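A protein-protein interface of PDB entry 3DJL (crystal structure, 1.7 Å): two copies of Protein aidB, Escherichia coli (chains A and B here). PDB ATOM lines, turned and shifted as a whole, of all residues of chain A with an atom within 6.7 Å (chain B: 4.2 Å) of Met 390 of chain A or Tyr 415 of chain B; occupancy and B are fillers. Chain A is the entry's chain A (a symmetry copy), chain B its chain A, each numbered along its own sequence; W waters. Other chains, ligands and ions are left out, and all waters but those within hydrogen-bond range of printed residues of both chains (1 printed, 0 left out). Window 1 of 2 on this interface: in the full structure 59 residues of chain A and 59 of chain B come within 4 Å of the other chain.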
ATOM      1  N   LEU A 261      28.603 -13.683 -39.851  1.00  0.00           N
ATOM      2  CA  LEU A 261      28.312 -12.747 -38.778  1.00  0.00           C
ATOM      3  C   LEU A 261      29.592 -12.240 -38.109  1.00  0.00           C
ATOM      4  O   LEU A 261      29.769 -11.037 -37.964  1.00  0.00           O
ATOM      5  CB  LEU A 261      27.458 -13.437 -37.735  1.00  0.00           C
ATOM      6  CG  LEU A 261      27.249 -12.758 -36.365  1.00  0.00           C
ATOM      7  CD1 LEU A 261      26.647 -11.341 -36.558  1.00  0.00           C
ATOM      8  CD2 LEU A 261      26.338 -13.610 -35.450  1.00  0.00           C
ATOM      9  N   SER A 306      36.117 -18.762 -25.917  1.00  0.00           N
ATOM     10  CA  SER A 306      35.000 -17.947 -25.402  1.00  0.00           C
ATOM     11  C   SER A 306      35.397 -17.321 -24.058  1.00  0.00           C
ATOM     12  O   SER A 306      35.109 -16.150 -23.830  1.00  0.00           O
ATOM     13  CB  SER A 306      33.715 -18.768 -25.221  1.00  0.00           C
ATOM     14  OG  SER A 306      33.289 -19.215 -26.509  1.00  0.00           O
ATOM     15  N   MET A 310      35.504 -13.307 -23.262  1.00  0.00           N
ATOM     16  CA  MET A 310      34.832 -12.782 -22.059  1.00  0.00           C
ATOM     17  C   MET A 310      35.829 -11.971 -21.164  1.00  0.00           C
ATOM     18  O   MET A 310      35.513 -10.878 -20.711  1.00  0.00           O
ATOM     19  CB  MET A 310      34.185 -13.916 -21.240  1.00  0.00           C
ATOM     20  CG  MET A 310      33.058 -14.560 -22.058  1.00  0.00           C
ATOM     21  SD  MET A 310      32.615 -16.175 -21.304  1.00  0.00           S
ATOM     22  CE  MET A 310      31.614 -15.702 -19.987  1.00  0.00           C
ATOM     23  N   ILE A 385      30.348 -22.638 -21.026  1.00  0.00           N
ATOM     24  CA  ILE A 385      31.138 -21.429 -21.250  1.00  0.00           C
ATOM     25  C   ILE A 385      30.784 -20.768 -22.579  1.00  0.00           C
ATOM     26  O   ILE A 385      30.568 -19.575 -22.629  1.00  0.00           O
ATOM     27  CB  ILE A 385      32.654 -21.685 -21.101  1.00  0.00           C
ATOM     28  CG1 ILE A 385      32.923 -22.092 -19.652  1.00  0.00           C
ATOM     29  CG2 ILE A 385      33.383 -20.371 -21.498  1.00  0.00           C
ATOM     30  CD1 ILE A 385      34.364 -22.476 -19.303  1.00  0.00           C
ATOM     31  N   CYS A 386      30.640 -21.558 -23.629  1.00  0.00           N
ATOM     32  CA  CYS A 386      30.339 -20.980 -24.935  1.00  0.00           C
ATOM     33  C   CYS A 386      28.936 -20.366 -24.965  1.00  0.00           C
ATOM     34  O   CYS A 386      28.695 -19.385 -25.629  1.00  0.00           O
ATOM     35  CB  CYS A 386      30.598 -22.013 -26.009  1.00  0.00           C
ATOM     36  SG  CYS A 386      32.388 -22.510 -26.055  1.00  0.00           S
ATOM     37  N   LYS A 387      28.004 -20.956 -24.215  1.00  0.00           N
ATOM     38  CA  LYS A 387      26.654 -20.412 -24.140  1.00  0.00           C
ATOM     39  C   LYS A 387      26.711 -19.105 -23.346  1.00  0.00           C
ATOM     40  O   LYS A 387      26.061 -18.129 -23.724  1.00  0.00           O
ATOM     41  CB  LYS A 387      25.723 -21.434 -23.458  1.00  0.00           C
ATOM     42  CG  LYS A 387      24.286 -21.385 -23.856  1.00  0.00           C
ATOM     43  CD  LYS A 387      24.161 -21.898 -25.248  1.00  0.00           C
ATOM     44  CE  LYS A 387      22.757 -22.286 -25.540  1.00  0.00           C
ATOM     45  NZ  LYS A 387      22.697 -22.749 -26.899  1.00  0.00           N
ATOM     46  N   ARG A 388      27.464 -19.064 -22.246  1.00  0.00           N
ATOM     47  CA  ARG A 388      27.581 -17.838 -21.422  1.00  0.00           C
ATOM     48  C   ARG A 388      28.174 -16.634 -22.171  1.00  0.00           C
ATOM     49  O   ARG A 388      27.994 -15.484 -21.755  1.00  0.00           O
ATOM     50  CB  ARG A 388      28.503 -18.104 -20.241  1.00  0.00           C
ATOM     51  CG  ARG A 388      27.866 -18.841 -19.104  1.00  0.00           C
ATOM     52  CD  ARG A 388      28.971 -19.102 -18.037  1.00  0.00           C
ATOM     53  NE  ARG A 388      28.474 -19.741 -16.825  1.00  0.00           N
ATOM     54  CZ  ARG A 388      29.233 -20.040 -15.771  1.00  0.00           C
ATOM     55  NH1 ARG A 388      30.539 -19.776 -15.791  1.00  0.00           N
ATOM     56  NH2 ARG A 388      28.689 -20.646 -14.718  1.00  0.00           N
ATOM     57  N   GLY A 389      28.956 -16.900 -23.207  1.00  0.00           N
ATOM     58  CA  GLY A 389      29.749 -15.867 -23.875  1.00  0.00           C
ATOM     59  C   GLY A 389      28.858 -14.736 -24.392  1.00  0.00           C
ATOM     60  O   GLY A 389      29.215 -13.568 -24.266  1.00  0.00           O
ATOM     61  N   MET A 390      27.716 -15.094 -24.977  1.00  0.00           N
ATOM     62  CA  MET A 390      26.882 -14.114 -25.655  1.00  0.00           C
ATOM     63  C   MET A 390      26.326 -13.112 -24.624  1.00  0.00           C
ATOM     64  O   MET A 390      26.546 -11.915 -24.752  1.00  0.00           O
ATOM     65  CB  MET A 390      25.767 -14.778 -26.510  1.00  0.00           C
ATOM     66  CG  MET A 390      26.261 -15.416 -27.825  1.00  0.00           C
ATOM     67  SD  MET A 390      27.173 -16.946 -27.584  1.00  0.00           S
ATOM     68  CE  MET A 390      25.831 -18.160 -27.175  1.00  0.00           C
ATOM     69  N   PRO A 391      25.596 -13.573 -23.600  1.00  0.00           N
ATOM     70  CA  PRO A 391      25.083 -12.549 -22.660  1.00  0.00           C
ATOM     71  C   PRO A 391      26.180 -11.809 -21.860  1.00  0.00           C
ATOM     72  O   PRO A 391      26.027 -10.626 -21.516  1.00  0.00           O
ATOM     73  CB  PRO A 391      24.214 -13.382 -21.693  1.00  0.00           C
ATOM     74  CG  PRO A 391      24.726 -14.778 -21.828  1.00  0.00           C
ATOM     75  CD  PRO A 391      25.076 -14.927 -23.271  1.00  0.00           C
ATOM     76  N   PHE A 392      27.283 -12.498 -21.619  1.00  0.00           N
ATOM     77  CA  PHE A 392      28.378 -11.886 -20.864  1.00  0.00           C
ATOM     78  C   PHE A 392      28.975 -10.713 -21.664  1.00  0.00           C
ATOM     79  O   PHE A 392      29.142  -9.625 -21.139  1.00  0.00           O
ATOM     80  CB  PHE A 392      29.428 -12.959 -20.531  1.00  0.00           C
ATOM     81  CG  PHE A 392      30.560 -12.451 -19.617  1.00  0.00           C
ATOM     82  CD1 PHE A 392      31.541 -11.613 -20.091  1.00  0.00           C
ATOM     83  CD2 PHE A 392      30.565 -12.797 -18.265  1.00  0.00           C
ATOM     84  CE1 PHE A 392      32.599 -11.147 -19.250  1.00  0.00           C
ATOM     85  CE2 PHE A 392      31.577 -12.374 -17.441  1.00  0.00           C
ATOM     86  CZ  PHE A 392      32.600 -11.541 -17.945  1.00  0.00           C
ATOM     87  N   VAL A 393      29.284 -10.927 -22.955  1.00  0.00           N
ATOM     88  CA  VAL A 393      29.854  -9.871 -23.766  1.00  0.00           C
ATOM     89  C   VAL A 393      28.843  -8.706 -24.004  1.00  0.00           C
ATOM     90  O   VAL A 393      29.211  -7.535 -23.992  1.00  0.00           O
ATOM     91  CB  VAL A 393      30.447 -10.431 -25.071  1.00  0.00           C
ATOM     92  CG1 VAL A 393      30.909  -9.297 -26.037  1.00  0.00           C
ATOM     93  CG2 VAL A 393      31.621 -11.373 -24.719  1.00  0.00           C
ATOM     94  N   ALA A 394      27.567  -9.038 -24.160  1.00  0.00           N
ATOM     95  CA  ALA A 394      26.523  -8.018 -24.284  1.00  0.00           C
ATOM     96  C   ALA A 394      26.486  -7.144 -23.042  1.00  0.00           C
ATOM     97  O   ALA A 394      26.190  -5.967 -23.129  1.00  0.00           O
ATOM     98  CB  ALA A 394      25.148  -8.669 -24.487  1.00  0.00           C
ATOM     99  N   GLU A 395      26.660  -7.750 -21.869  1.00  0.00           N
ATOM    100  CA  GLU A 395      26.655  -6.975 -20.656  1.00  0.00           C
ATOM    101  C   GLU A 395      27.852  -6.024 -20.646  1.00  0.00           C
ATOM    102  O   GLU A 395      27.721  -4.844 -20.311  1.00  0.00           O
ATOM    103  CB  GLU A 395      26.717  -7.878 -19.450  1.00  0.00           C
ATOM    104  CG  GLU A 395      26.605  -7.100 -18.165  1.00  0.00           C
ATOM    105  CD  GLU A 395      25.146  -6.733 -17.884  1.00  0.00           C
ATOM    106  OE1 GLU A 395      24.360  -7.655 -17.642  1.00  0.00           O
ATOM    107  OE2 GLU A 395      24.785  -5.547 -17.952  1.00  0.00           O
ATOM    108  N   TYR A 405      28.375  -0.084 -28.809  1.00  0.00           N
ATOM    109  CA  TYR A 405      27.585  -0.609 -29.938  1.00  0.00           C
ATOM    110  C   TYR A 405      28.187  -0.163 -31.311  1.00  0.00           C
ATOM    111  O   TYR A 405      27.682  -0.534 -32.370  1.00  0.00           O
ATOM    112  CB  TYR A 405      26.139  -0.089 -29.802  1.00  0.00           C
ATOM    113  CG  TYR A 405      25.126  -0.828 -30.688  1.00  0.00           C
ATOM    114  CD1 TYR A 405      24.545  -0.189 -31.778  1.00  0.00           C
ATOM    115  CD2 TYR A 405      24.755  -2.150 -30.389  1.00  0.00           C
ATOM    116  CE1 TYR A 405      23.592  -0.878 -32.598  1.00  0.00           C
ATOM    117  CE2 TYR A 405      23.859  -2.854 -31.191  1.00  0.00           C
ATOM    118  CZ  TYR A 405      23.249  -2.206 -32.258  1.00  0.00           C
ATOM    119  OH  TYR A 405      22.340  -2.908 -33.042  1.00  0.00           O
ATOM    120  N   LEU A 414      33.806  -8.761 -30.705  1.00  0.00           N
ATOM    121  CA  LEU A 414      33.724  -9.828 -29.680  1.00  0.00           C
ATOM    122  C   LEU A 414      32.320 -10.434 -29.661  1.00  0.00           C
ATOM    123  O   LEU A 414      32.143 -11.603 -29.740  1.00  0.00           O
ATOM    124  CB  LEU A 414      34.064  -9.265 -28.281  1.00  0.00           C
ATOM    125  CG  LEU A 414      35.545  -8.867 -28.133  1.00  0.00           C
ATOM    126  CD1 LEU A 414      35.765  -7.988 -26.853  1.00  0.00           C
ATOM    127  CD2 LEU A 414      36.415 -10.079 -28.102  1.00  0.00           C
ATOM    128  N   TYR A 415      31.316  -9.577 -29.605  1.00  0.00           N
ATOM    129  CA  TYR A 415      29.932 -10.013 -29.587  1.00  0.00           C
ATOM    130  C   TYR A 415      29.566 -10.838 -30.814  1.00  0.00           C
ATOM    131  O   TYR A 415      28.851 -11.867 -30.690  1.00  0.00           O
ATOM    132  CB  TYR A 415      29.060  -8.757 -29.554  1.00  0.00           C
ATOM    133  CG  TYR A 415      27.544  -9.033 -29.486  1.00  0.00           C
ATOM    134  CD1 TYR A 415      26.947  -9.602 -28.342  1.00  0.00           C
ATOM    135  CD2 TYR A 415      26.753  -8.823 -30.605  1.00  0.00           C
ATOM    136  CE1 TYR A 415      25.545  -9.869 -28.356  1.00  0.00           C
ATOM    137  CE2 TYR A 415      25.408  -9.061 -30.606  1.00  0.00           C
ATOM    138  CZ  TYR A 415      24.804  -9.580 -29.496  1.00  0.00           C
ATOM    139  OH  TYR A 415      23.422  -9.797 -29.553  1.00  0.00           O
ATOM    140  N   ARG A 416      30.045 -10.415 -31.987  1.00  0.00           N
ATOM    141  CA  ARG A 416      29.690 -11.129 -33.211  1.00  0.00           C
ATOM    142  C   ARG A 416      30.444 -12.478 -33.291  1.00  0.00           C
ATOM    143  O   ARG A 416      29.989 -13.392 -33.991  1.00  0.00           O
ATOM    144  CB  ARG A 416      30.041 -10.298 -34.449  1.00  0.00           C
ATOM    145  CG  ARG A 416      29.081  -9.118 -34.622  1.00  0.00           C
ATOM    146  CD  ARG A 416      29.364  -8.377 -35.971  1.00  0.00           C
ATOM    147  NE  ARG A 416      30.533  -7.488 -35.906  1.00  0.00           N
ATOM    148  CZ  ARG A 416      31.706  -7.803 -36.435  1.00  0.00           C
ATOM    149  NH1 ARG A 416      31.877  -8.992 -36.971  1.00  0.00           N
ATOM    150  NH2 ARG A 416      32.744  -6.946 -36.339  1.00  0.00           N
ATOM    151  N   GLU A 417      31.587 -12.576 -32.603  1.00  0.00           N
ATOM    152  CA  GLU A 417      32.346 -13.850 -32.572  1.00  0.00           C
ATOM    153  C   GLU A 417      31.710 -14.914 -31.683  1.00  0.00           C
ATOM    154  O   GLU A 417      31.800 -16.110 -32.001  1.00  0.00           O
ATOM    155  CB  GLU A 417      33.783 -13.599 -32.119  1.00  0.00           C
ATOM    156  CG  GLU A 417      34.708 -14.766 -32.348  1.00  0.00           C
ATOM    157  CD  GLU A 417      35.198 -14.798 -33.794  1.00  0.00           C
ATOM    158  OE1 GLU A 417      35.618 -15.881 -34.249  1.00  0.00           O
ATOM    159  OE2 GLU A 417      35.143 -13.735 -34.463  1.00  0.00           O
ATOM    160  N   MET A 418      31.062 -14.511 -30.590  1.00  0.00           N
ATOM    161  CA  MET A 418      30.709 -15.452 -29.518  1.00  0.00           C
ATOM    162  C   MET A 418      29.913 -16.702 -29.998  1.00  0.00           C
ATOM    163  O   MET A 418      30.229 -17.845 -29.565  1.00  0.00           O
ATOM    164  CB  MET A 418      29.982 -14.754 -28.350  1.00  0.00           C
ATOM    165  CG  MET A 418      30.745 -13.537 -27.729  1.00  0.00           C
ATOM    166  SD  MET A 418      32.507 -13.880 -27.400  1.00  0.00           S
ATOM    167  CE  MET A 418      32.382 -15.028 -26.024  1.00  0.00           C
ATOM    168  N   PRO A 419      28.926 -16.525 -30.923  1.00  0.00           N
ATOM    169  CA  PRO A 419      28.135 -17.727 -31.282  1.00  0.00           C
ATOM    170  C   PRO A 419      28.897 -18.831 -31.997  1.00  0.00           C
ATOM    171  O   PRO A 419      28.459 -19.988 -31.979  1.00  0.00           O
ATOM    172  CB  PRO A 419      27.043 -17.163 -32.213  1.00  0.00           C
ATOM    173  CG  PRO A 419      26.884 -15.770 -31.800  1.00  0.00           C
ATOM    174  CD  PRO A 419      28.308 -15.302 -31.447  1.00  0.00           C
ATOM    175  N   VAL A 420      29.978 -18.490 -32.693  1.00  0.00           N
ATOM    176  CA  VAL A 420      30.674 -19.486 -33.490  1.00  0.00           C
ATOM    177  C   VAL A 420      31.167 -20.613 -32.591  1.00  0.00           C
ATOM    178  O   VAL A 420      31.099 -21.792 -32.945  1.00  0.00           O
ATOM    179  CB  VAL A 420      31.798 -18.838 -34.358  1.00  0.00           C
ATOM    180  CG1 VAL A 420      33.024 -18.601 -33.581  1.00  0.00           C
ATOM    181  CG2 VAL A 420      32.107 -19.741 -35.528  1.00  0.00           C
ATOM    182  N   SER A 422      29.925 -21.592 -29.884  1.00  0.00           N
ATOM    183  CA  SER A 422      28.789 -22.383 -29.395  1.00  0.00           C
ATOM    184  C   SER A 422      28.252 -23.369 -30.491  1.00  0.00           C
ATOM    185  O   SER A 422      27.756 -24.444 -30.197  1.00  0.00           O
ATOM    186  CB  SER A 422      27.710 -21.433 -28.808  1.00  0.00           C
ATOM    187  OG  SER A 422      26.812 -22.184 -28.015  1.00  0.00           O
ATOM    188  N   VAL B 393      17.932 -15.067 -29.065  1.00  0.00           N
ATOM    189  CA  VAL B 393      18.186 -15.080 -30.490  1.00  0.00           C
ATOM    190  C   VAL B 393      19.420 -15.963 -30.856  1.00  0.00           C
ATOM    191  O   VAL B 393      19.416 -16.673 -31.857  1.00  0.00           O
ATOM    192  CB  VAL B 393      18.280 -13.651 -31.052  1.00  0.00           C
ATOM    193  CG1 VAL B 393      18.725 -13.638 -32.547  1.00  0.00           C
ATOM    194  CG2 VAL B 393      16.912 -12.955 -30.874  1.00  0.00           C
ATOM    195  N   ALA B 394      20.441 -15.954 -30.007  1.00  0.00           N
ATOM    196  CA  ALA B 394      21.602 -16.827 -30.201  1.00  0.00           C
ATOM    197  C   ALA B 394      21.177 -18.285 -30.188  1.00  0.00           C
ATOM    198  O   ALA B 394      21.759 -19.099 -30.880  1.00  0.00           O
ATOM    199  CB  ALA B 394      22.647 -16.594 -29.101  1.00  0.00           C
ATOM    200  N   MET B 397      19.623 -19.161 -33.466  1.00  0.00           N
ATOM    201  CA  MET B 397      20.659 -19.263 -34.479  1.00  0.00           C
ATOM    202  C   MET B 397      21.286 -20.674 -34.389  1.00  0.00           C
ATOM    203  O   MET B 397      21.533 -21.314 -35.384  1.00  0.00           O
ATOM    204  CB  MET B 397      21.741 -18.213 -34.180  1.00  0.00           C
ATOM    205  CG  MET B 397      22.824 -18.206 -35.175  1.00  0.00           C
ATOM    206  SD  MET B 397      24.051 -16.928 -34.670  1.00  0.00           S
ATOM    207  CE  MET B 397      23.162 -15.486 -35.022  1.00  0.00           C
ATOM    208  N   LEU B 411      18.957 -14.380 -39.184  1.00  0.00           N
ATOM    209  CA  LEU B 411      19.375 -14.505 -37.780  1.00  0.00           C
ATOM    210  C   LEU B 411      20.505 -13.584 -37.358  1.00  0.00           C
ATOM    211  O   LEU B 411      20.401 -12.987 -36.313  1.00  0.00           O
ATOM    212  CB  LEU B 411      19.675 -15.952 -37.396  1.00  0.00           C
ATOM    213  CG  LEU B 411      18.471 -16.760 -36.833  1.00  0.00           C
ATOM    214  CD1 LEU B 411      18.054 -16.188 -35.473  1.00  0.00           C
ATOM    215  CD2 LEU B 411      17.309 -16.725 -37.723  1.00  0.00           C
ATOM    216  N   PRO B 412      21.568 -13.434 -38.177  1.00  0.00           N
ATOM    217  CA  PRO B 412      22.618 -12.513 -37.758  1.00  0.00           C
ATOM    218  C   PRO B 412      22.090 -11.076 -37.556  1.00  0.00           C
ATOM    219  O   PRO B 412      22.484 -10.406 -36.569  1.00  0.00           O
ATOM    220  CB  PRO B 412      23.622 -12.606 -38.920  1.00  0.00           C
ATOM    221  CG  PRO B 412      23.520 -14.097 -39.242  1.00  0.00           C
ATOM    222  CD  PRO B 412      22.021 -14.288 -39.294  1.00  0.00           C
ATOM    223  N   ARG B 413      21.285 -10.591 -38.505  1.00  0.00           N
ATOM    224  CA  ARG B 413      20.751  -9.210 -38.355  1.00  0.00           C
ATOM    225  C   ARG B 413      19.932  -9.059 -37.047  1.00  0.00           C
ATOM    226  O   ARG B 413      20.123  -8.083 -36.338  1.00  0.00           O
ATOM    227  CB  ARG B 413      19.898  -8.818 -39.575  1.00  0.00           C
ATOM    228  CG  ARG B 413      19.255  -7.458 -39.400  1.00  0.00           C
ATOM    229  CD  ARG B 413      18.882  -6.837 -40.814  1.00  0.00           C
ATOM    230  NE  ARG B 413      18.231  -7.799 -41.673  1.00  0.00           N
ATOM    231  CZ  ARG B 413      16.920  -7.910 -41.838  1.00  0.00           C
ATOM    232  NH1 ARG B 413      16.045  -7.092 -41.206  1.00  0.00           N
ATOM    233  NH2 ARG B 413      16.481  -8.843 -42.645  1.00  0.00           N
ATOM    234  N   LEU B 414      19.087 -10.050 -36.727  1.00  0.00           N
ATOM    235  CA  LEU B 414      18.323 -10.053 -35.457  1.00  0.00           C
ATOM    236  C   LEU B 414      19.282 -10.010 -34.266  1.00  0.00           C
ATOM    237  O   LEU B 414      19.170  -9.208 -33.402  1.00  0.00           O
ATOM    238  CB  LEU B 414      17.433 -11.313 -35.360  1.00  0.00           C
ATOM    239  CG  LEU B 414      16.270 -11.310 -36.370  1.00  0.00           C
ATOM    240  CD1 LEU B 414      15.620 -12.732 -36.483  1.00  0.00           C
ATOM    241  CD2 LEU B 414      15.249 -10.287 -35.994  1.00  0.00           C
ATOM    242  N   TYR B 415      20.272 -10.886 -34.283  1.00  0.00           N
ATOM    243  CA  TYR B 415      21.258 -10.954 -33.220  1.00  0.00           C
ATOM    244  C   TYR B 415      22.009  -9.641 -33.040  1.00  0.00           C
ATOM    245  O   TYR B 415      22.252  -9.209 -31.882  1.00  0.00           O
ATOM    246  CB  TYR B 415      22.255 -12.050 -33.595  1.00  0.00           C
ATOM    247  CG  TYR B 415      23.360 -12.295 -32.547  1.00  0.00           C
ATOM    248  CD1 TYR B 415      23.070 -12.848 -31.282  1.00  0.00           C
ATOM    249  CD2 TYR B 415      24.655 -11.867 -32.796  1.00  0.00           C
ATOM    250  CE1 TYR B 415      24.131 -13.013 -30.341  1.00  0.00           C
ATOM    251  CE2 TYR B 415      25.671 -12.046 -31.900  1.00  0.00           C
ATOM    252  CZ  TYR B 415      25.418 -12.611 -30.683  1.00  0.00           C
ATOM    253  OH  TYR B 415      26.498 -12.776 -29.808  1.00  0.00           O
ATOM    254  N   ARG B 416      22.372  -8.999 -34.152  1.00  0.00           N
ATOM    255  CA  ARG B 416      23.141  -7.761 -34.054  1.00  0.00           C
ATOM    256  C   ARG B 416      22.240  -6.598 -33.573  1.00  0.00           C
ATOM    257  O   ARG B 416      22.753  -5.611 -33.030  1.00  0.00           O
ATOM    258  CB  ARG B 416      23.746  -7.383 -35.410  1.00  0.00           C
ATOM    259  CG  ARG B 416      24.907  -8.309 -35.783  1.00  0.00           C
ATOM    260  CD  ARG B 416      25.603  -7.811 -37.093  1.00  0.00           C
ATOM    261  NE  ARG B 416      24.859  -8.163 -38.310  1.00  0.00           N
ATOM    262  CZ  ARG B 416      24.128  -7.287 -38.985  1.00  0.00           C
ATOM    263  NH1 ARG B 416      23.982  -6.067 -38.516  1.00  0.00           N
ATOM    264  NH2 ARG B 416      23.465  -7.671 -40.095  1.00  0.00           N
ATOM    265  N   GLU B 417      20.926  -6.716 -33.799  1.00  0.00           N
ATOM    266  CA  GLU B 417      19.980  -5.679 -33.319  1.00  0.00           C
ATOM    267  C   GLU B 417      19.734  -5.731 -31.815  1.00  0.00           C
ATOM    268  O   GLU B 417      19.532  -4.676 -31.192  1.00  0.00           O
ATOM    269  CB  GLU B 417      18.648  -5.798 -34.058  1.00  0.00           C
ATOM    270  CG  GLU B 417      17.737  -4.613 -33.868  1.00  0.00           C
ATOM    271  CD  GLU B 417      18.125  -3.470 -34.804  1.00  0.00           C
ATOM    272  OE1 GLU B 417      17.761  -2.315 -34.504  1.00  0.00           O
ATOM    273  OE2 GLU B 417      18.803  -3.745 -35.827  1.00  0.00           O
ATOM    274  N   MET B 418      19.760  -6.922 -31.217  1.00  0.00           N
ATOM    275  CA  MET B 418      19.219  -7.111 -29.863  1.00  0.00           C
ATOM    276  C   MET B 418      19.800  -6.133 -28.798  1.00  0.00           C
ATOM    277  O   MET B 418      19.021  -5.575 -27.976  1.00  0.00           O
ATOM    278  CB  MET B 418      19.341  -8.574 -29.389  1.00  0.00           C
ATOM    279  CG  MET B 418      18.702  -9.634 -30.346  1.00  0.00           C
ATOM    280  SD  MET B 418      17.027  -9.181 -30.912  1.00  0.00           S
ATOM    281  CE  MET B 418      16.087  -9.381 -29.395  1.00  0.00           C
ATOM    282  N   PRO B 419      21.138  -5.867 -28.826  1.00  0.00           N
ATOM    283  CA  PRO B 419      21.660  -5.004 -27.738  1.00  0.00           C
ATOM    284  C   PRO B 419      21.160  -3.568 -27.735  1.00  0.00           C
ATOM    285  O   PRO B 419      21.207  -2.906 -26.690  1.00  0.00           O
ATOM    286  CB  PRO B 419      23.183  -5.023 -27.978  1.00  0.00           C
ATOM    287  CG  PRO B 419      23.439  -6.294 -28.654  1.00  0.00           C
ATOM    288  CD  PRO B 419      22.227  -6.493 -29.583  1.00  0.00           C
HETATM  289  O   HOH W   1      23.052 -20.221 -27.831  1.00  0.00           O
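The backbone carbonyl oxygen (O) of Arg 416 of chain B lies within hydrogen-bond range of the side-chain hydroxyl (OH) of Tyr 405 of chain A (2.7 Å). The side-chain hydroxyl of Tyr 415 of chain B is in hydrogen-bond range of the backbone carbonyl oxygen of Tyr 415 of chain A.
The guanidinium group (NH1) of Arg 416 of chain A sits at hydrogen-bond distance from the backbone carbonyl oxygen (O) of Leu 261 of chain A, at 3.1 Å.
Met 397 of chain B touches Leu 261 of chain A (CE to CD2, 3.7 Å). Tyr 415 of chain B touches Leu 261 of chain A (CD2 to CD2, 3.6 Å). Arg 416 of chain B touches Leu 261 of chain A (CG to CD1, 3.6 Å). CG of Met 390 of chain A touches OH of Tyr 415 of chain B, 3.3 Å away. OH of Tyr 405 of chain A touches CA of Glu 417 of chain B, 3.7 Å away. Pro 419 of chain B touches Tyr 405 of chain A. Tyr 415 of chain A touches Pro 419 of chain B. Arg 416 of chain A touches Arg 416 of chain B. Met 397 of chain B touches Pro 419 of chain A (SD to CB, 3.9 Å). Tyr 415 of chain B touches Pro 419 of chain A.
Of the printed residues of chain B, Met 390 of chain A touches Tyr 415. Tyr 415 of chain B touches just these residues of chain A: Leu 261, Met 390, Tyr 415 and Pro 419. Printed residues of chain A within 4 Å of Pro 419 of chain B: Tyr 405 and Tyr 415. Of the printed residues of chain A, Arg 416 of chain B touches Leu 261, Tyr 405 and Arg 416. Printed residues of chain B within 4 Å of Tyr 415 of chain A: Tyr 415 (2.7 Å) and Pro 419 (3.5 Å). Printed residues of chain B within 4 Å of Leu 261 of chain A: Met 397 (3.7 Å), Tyr 415 (3.6 Å) and Arg 416 (3.6 Å). Leu 414 of chain A touches none of the printed residues of chain B. The nearest printed residue of chain B that does not touch Met 390 of chain A is Ala 394 of chain B (4.01 Å). The nearest residue of chain A that does not touch Tyr 415 of chain B is Met 418 of chain A (4.3 Å).
Hydrophobic or aromatic side chains of chain A within 4 Å of the printed part of chain B: Leu 261, Met 390, Tyr 405, Tyr 415 and Pro 419. Of the 12 printed residues of chain B, 5 touch a printed residue of chain A. Printed residues of chain B that touch a printed residue of chain A: Met 397, Tyr 415, Arg 416, Glu 417 and Pro 419. Hydrophobic or aromatic side chains of chain B within 4 Å of the printed part of chain A: Met 397, Tyr 415 and Pro 419. Among the printed residues, 12 pairs touch across the chains. Among the printed residues, no Asp or Glu carboxylate lies within 4 Å of a Lys or Arg side-chain nitrogen of the other chain.
Tyr 415 of chain B touches its own counterpart, Tyr 415 of chain A. Tyr 415 of chain A touches Pro 419 of chain B, and with the chains exchanged Pro 419 of chain A touches Tyr 415 of chain B. Arg 416 of chain B touches its own counterpart, Arg 416 of chain A. Of the 12 pairs that touch across the chains among the printed residues, 4 have their exchanged pair printed and touching as well.
Water W1 lies within hydrogen-bond range of the side-chain amino group of Lys 387 of chain A and the backbone carbonyl oxygen of Ala 394 of chain B.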
